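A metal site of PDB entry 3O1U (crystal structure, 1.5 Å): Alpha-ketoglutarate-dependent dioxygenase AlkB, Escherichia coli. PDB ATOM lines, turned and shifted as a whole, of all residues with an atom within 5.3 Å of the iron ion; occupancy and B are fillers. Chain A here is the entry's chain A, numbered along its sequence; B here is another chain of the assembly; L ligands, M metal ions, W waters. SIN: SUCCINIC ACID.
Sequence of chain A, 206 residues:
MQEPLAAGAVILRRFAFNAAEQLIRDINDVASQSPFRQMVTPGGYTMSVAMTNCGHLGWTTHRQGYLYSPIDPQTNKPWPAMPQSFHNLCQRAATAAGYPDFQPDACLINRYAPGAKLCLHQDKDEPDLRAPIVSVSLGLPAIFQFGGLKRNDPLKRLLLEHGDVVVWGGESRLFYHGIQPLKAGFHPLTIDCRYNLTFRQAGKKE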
ATOM      1  N   LEU A 118       7.193   3.884 -16.430  1.00  0.00           N
ATOM      2  CA  LEU A 118       6.577   3.349 -15.254  1.00  0.00           C
ATOM      3  C   LEU A 118       6.983   1.900 -15.192  1.00  0.00           C
ATOM      4  O   LEU A 118       6.559   1.099 -16.029  1.00  0.00           O
ATOM      5  CB  LEU A 118       5.053   3.466 -15.333  1.00  0.00           C
ATOM      6  CG  LEU A 118       4.278   3.344 -14.036  1.00  0.00           C
ATOM      7  CD1 LEU A 118       4.802   4.359 -13.022  1.00  0.00           C
ATOM      8  CD2 LEU A 118       2.791   3.527 -14.271  1.00  0.00           C
ATOM      9  N   HIS A 121       4.580  -3.095 -12.380  1.00  0.00           N
ATOM     10  CA  HIS A 121       3.914  -3.123 -11.098  1.00  0.00           C
ATOM     11  C   HIS A 121       2.555  -3.773 -11.284  1.00  0.00           C
ATOM     12  O   HIS A 121       2.128  -4.030 -12.410  1.00  0.00           O
ATOM     13  CB  HIS A 121       3.712  -1.690 -10.586  1.00  0.00           C
ATOM     14  CG  HIS A 121       2.777  -0.896 -11.420  1.00  0.00           C
ATOM     15  ND1 HIS A 121       3.174  -0.233 -12.565  1.00  0.00           N
ATOM     16  CD2 HIS A 121       1.444  -0.678 -11.304  1.00  0.00           C
ATOM     17  CE1 HIS A 121       2.122   0.351 -13.111  1.00  0.00           C
ATOM     18  NE2 HIS A 121       1.066   0.130 -12.351  1.00  0.00           N
ATOM     19  N   GLN A 122       1.886  -4.037 -10.169  1.00  0.00           N
ATOM     20  CA  GLN A 122       0.527  -4.550 -10.173  1.00  0.00           C
ATOM     21  C   GLN A 122      -0.404  -3.448  -9.679  1.00  0.00           C
ATOM     22  O   GLN A 122      -0.013  -2.631  -8.850  1.00  0.00           O
ATOM     23  CB  GLN A 122       0.409  -5.739  -9.222  1.00  0.00           C
ATOM     24  CG  GLN A 122       1.140  -7.013  -9.629  1.00  0.00           C
ATOM     25  CD  GLN A 122       1.106  -8.081  -8.544  1.00  0.00           C
ATOM     26  OE1 GLN A 122       1.674  -7.907  -7.465  1.00  0.00           O
ATOM     27  NE2 GLN A 122       0.432  -9.192  -8.834  1.00  0.00           N
ATOM     28  N   ASP A 123      -1.631  -3.421 -10.186  1.00  0.00           N
ATOM     29  CA  ASP A 123      -2.669  -2.571  -9.622  1.00  0.00           C
ATOM     30  C   ASP A 123      -3.313  -3.400  -8.534  1.00  0.00           C
ATOM     31  O   ASP A 123      -4.114  -4.290  -8.826  1.00  0.00           O
ATOM     32  CB  ASP A 123      -3.713  -2.214 -10.674  1.00  0.00           C
ATOM     33  CG  ASP A 123      -3.238  -1.146 -11.627  1.00  0.00           C
ATOM     34  OD1 ASP A 123      -2.013  -0.874 -11.694  1.00  0.00           O
ATOM     35  OD2 ASP A 123      -4.097  -0.567 -12.305  1.00  0.00           O
ATOM     36  N   TRP A 168      -8.211  -4.444 -18.577  1.00  0.00           N
ATOM     37  CA  TRP A 168      -7.900  -5.754 -18.003  1.00  0.00           C
ATOM     38  C   TRP A 168      -8.669  -6.051 -16.712  1.00  0.00           C
ATOM     39  O   TRP A 168      -9.074  -5.162 -15.979  1.00  0.00           O
ATOM     40  CB  TRP A 168      -6.390  -6.027 -17.900  1.00  0.00           C
ATOM     41  CG  TRP A 168      -5.573  -5.148 -16.973  1.00  0.00           C
ATOM     42  CD1 TRP A 168      -5.158  -5.477 -15.709  1.00  0.00           C
ATOM     43  CD2 TRP A 168      -5.036  -3.853 -17.248  1.00  0.00           C
ATOM     44  NE1 TRP A 168      -4.406  -4.464 -15.179  1.00  0.00           N
ATOM     45  CE2 TRP A 168      -4.308  -3.453 -16.106  1.00  0.00           C
ATOM     46  CE3 TRP A 168      -5.092  -2.996 -18.347  1.00  0.00           C
ATOM     47  CZ2 TRP A 168      -3.656  -2.236 -16.030  1.00  0.00           C
ATOM     48  CZ3 TRP A 168      -4.446  -1.786 -18.281  1.00  0.00           C
ATOM     49  CH2 TRP A 168      -3.739  -1.410 -17.117  1.00  0.00           C
ATOM     50  N   HIS A 177       2.406  -4.797 -15.319  1.00  0.00           N
ATOM     51  CA  HIS A 177       2.369  -3.958 -16.499  1.00  0.00           C
ATOM     52  C   HIS A 177       3.200  -2.716 -16.245  1.00  0.00           C
ATOM     53  O   HIS A 177       3.514  -2.386 -15.092  1.00  0.00           O
ATOM     54  CB  HIS A 177       0.922  -3.572 -16.832  1.00  0.00           C
ATOM     55  CG  HIS A 177       0.213  -2.891 -15.699  1.00  0.00           C
ATOM     56  ND1 HIS A 177      -0.332  -3.568 -14.630  1.00  0.00           N
ATOM     57  CD2 HIS A 177      -0.034  -1.582 -15.468  1.00  0.00           C
ATOM     58  CE1 HIS A 177      -0.876  -2.717 -13.780  1.00  0.00           C
ATOM     59  NE2 HIS A 177      -0.715  -1.502 -14.275  1.00  0.00           N
ATOM     60  N   ARG A 200     -10.591   2.893 -12.037  1.00  0.00           N
ATOM     61  CA  ARG A 200     -10.683   1.735 -11.148  1.00  0.00           C
ATOM     62  C   ARG A 200     -11.843   1.881 -10.181  1.00  0.00           C
ATOM     63  O   ARG A 200     -12.345   2.962  -9.955  1.00  0.00           O
ATOM     64  CB  ARG A 200      -9.409   1.573 -10.313  1.00  0.00           C
ATOM     65  CG  ARG A 200      -8.114   1.568 -11.106  1.00  0.00           C
ATOM     66  CD  ARG A 200      -6.917   1.164 -10.209  1.00  0.00           C
ATOM     67  NE  ARG A 200      -5.711   1.147 -11.011  1.00  0.00           N
ATOM     68  CZ  ARG A 200      -5.118   2.245 -11.473  1.00  0.00           C
ATOM     69  NH1 ARG A 200      -5.620   3.442 -11.201  1.00  0.00           N
ATOM     70  NH2 ARG A 200      -4.020   2.148 -12.220  1.00  0.00           N
ATOM     71  P   MDV B   7       6.324  -1.284  -7.314  1.00  0.00           P
ATOM     72  N1  MDV B   7      -0.077   2.815 -10.154  1.00  0.00           N
ATOM     73  C2  MDV B   7       0.856   3.519 -10.728  1.00  0.00           C
ATOM     74  N3  MDV B   7       2.129   3.327 -10.396  1.00  0.00           N
ATOM     75  C4  MDV B   7       2.430   2.352  -9.475  1.00  0.00           C
ATOM     76  C5  MDV B   7       1.446   1.608  -8.866  1.00  0.00           C
ATOM     77  C6  MDV B   7       0.143   1.855  -9.257  1.00  0.00           C
ATOM     78  N6  MDV B   7      -0.952   1.226  -8.786  1.00  0.00           N
ATOM     79  N7  MDV B   7       2.041   0.738  -8.018  1.00  0.00           N
ATOM     80  C8  MDV B   7       3.373   0.957  -8.101  1.00  0.00           C
ATOM     81  N9  MDV B   7       3.581   1.974  -8.959  1.00  0.00           N
ATOM     82  C1' MDV B   7       4.861   2.506  -9.430  1.00  0.00           C
ATOM     83  O1P MDV B   7       5.467  -0.881  -6.144  1.00  0.00           O
ATOM     84  C2' MDV B   7       5.948   2.765  -8.388  1.00  0.00           C
ATOM     85  C22 MDV B   7      -1.443   2.547 -10.597  1.00  0.00           C
ATOM     86  C23 MDV B   7      -2.112   1.641  -9.566  1.00  0.00           C
ATOM     87  O26 MDV B   7      -2.941   2.498  -8.801  1.00  0.00           O
ATOM     88  O2P MDV B   7       5.799  -2.374  -8.242  1.00  0.00           O
ATOM     89  C3' MDV B   7       7.185   2.571  -9.273  1.00  0.00           C
ATOM     90  O3' MDV B   7       7.360   3.732 -10.113  1.00  0.00           O
ATOM     91  C4' MDV B   7       6.811   1.414 -10.157  1.00  0.00           C
ATOM     92  O4' MDV B   7       5.378   1.489 -10.289  1.00  0.00           O
ATOM     93  C5' MDV B   7       7.168   0.091  -9.483  1.00  0.00           C
ATOM     94  O5' MDV B   7       6.534   0.055  -8.198  1.00  0.00           O
ATOM     95  O24 MDV B   7      -1.468   1.960 -12.119  1.00  0.00           O
HETATM   96  C1  SIN L   1      -0.618   2.949 -14.939  1.00  0.00           C
HETATM   97  O1  SIN L   1      -0.332   1.736 -14.822  1.00  0.00           O
HETATM   98  O2  SIN L   1      -1.081   3.590 -13.960  1.00  0.00           O
HETATM   99  C2  SIN L   1      -0.384   3.654 -16.252  1.00  0.00           C
HETATM  100  C3  SIN L   1      -0.118   2.718 -17.410  1.00  0.00           C
HETATM  101  C4  SIN L   1      -0.082   3.581 -18.669  1.00  0.00           C
HETATM  102  O3  SIN L   1       0.392   4.731 -18.619  1.00  0.00           O
HETATM  103  O4  SIN L   1      -0.513   3.154 -19.758  1.00  0.00           O
HETATM  104 FE    FE M   1      -0.944   0.350 -13.204  1.00  0.00          FE
HETATM  105  O   HOH W   1      -2.971   0.471 -14.234  1.00  0.00           O
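Residues that only touch the iron ion: Arg 200.
The nearest printed residue that does not touch the iron ion is Trp 168 (4.7 Å).
Water W1 lies within hydrogen-bond range of the side-chain carboxylate (OD2) of Asp 123 (2.5 Å) and the guanidinium group (NH2) of Arg 200 (2.8 Å).
The iron ion is bound by O24 of MDV 7 of chain B (2.0 Å).
A ring nitrogen (NE2) of His 177 is bound to the iron ion.
A ring nitrogen (NE2) of His 121 binds the iron ion, at 2.2 Å.
O1 of the ligand is bound to the iron ion (2.2 Å).
The side-chain carboxylate (OD1) of Asp 123 is bound to the iron ion (2.2 Å).
Water W1 is bound to the iron ion (2.3 Å).
The iron ion has six donor atoms within binding distance.
The guanidinium group of Arg 200 lies within salt-bridge range of the side-chain carboxylate of Asp 123.
The guanidinium group (NH2) of Arg 200 lies close to O24 of MDV 7 of chain B (2.6 Å).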
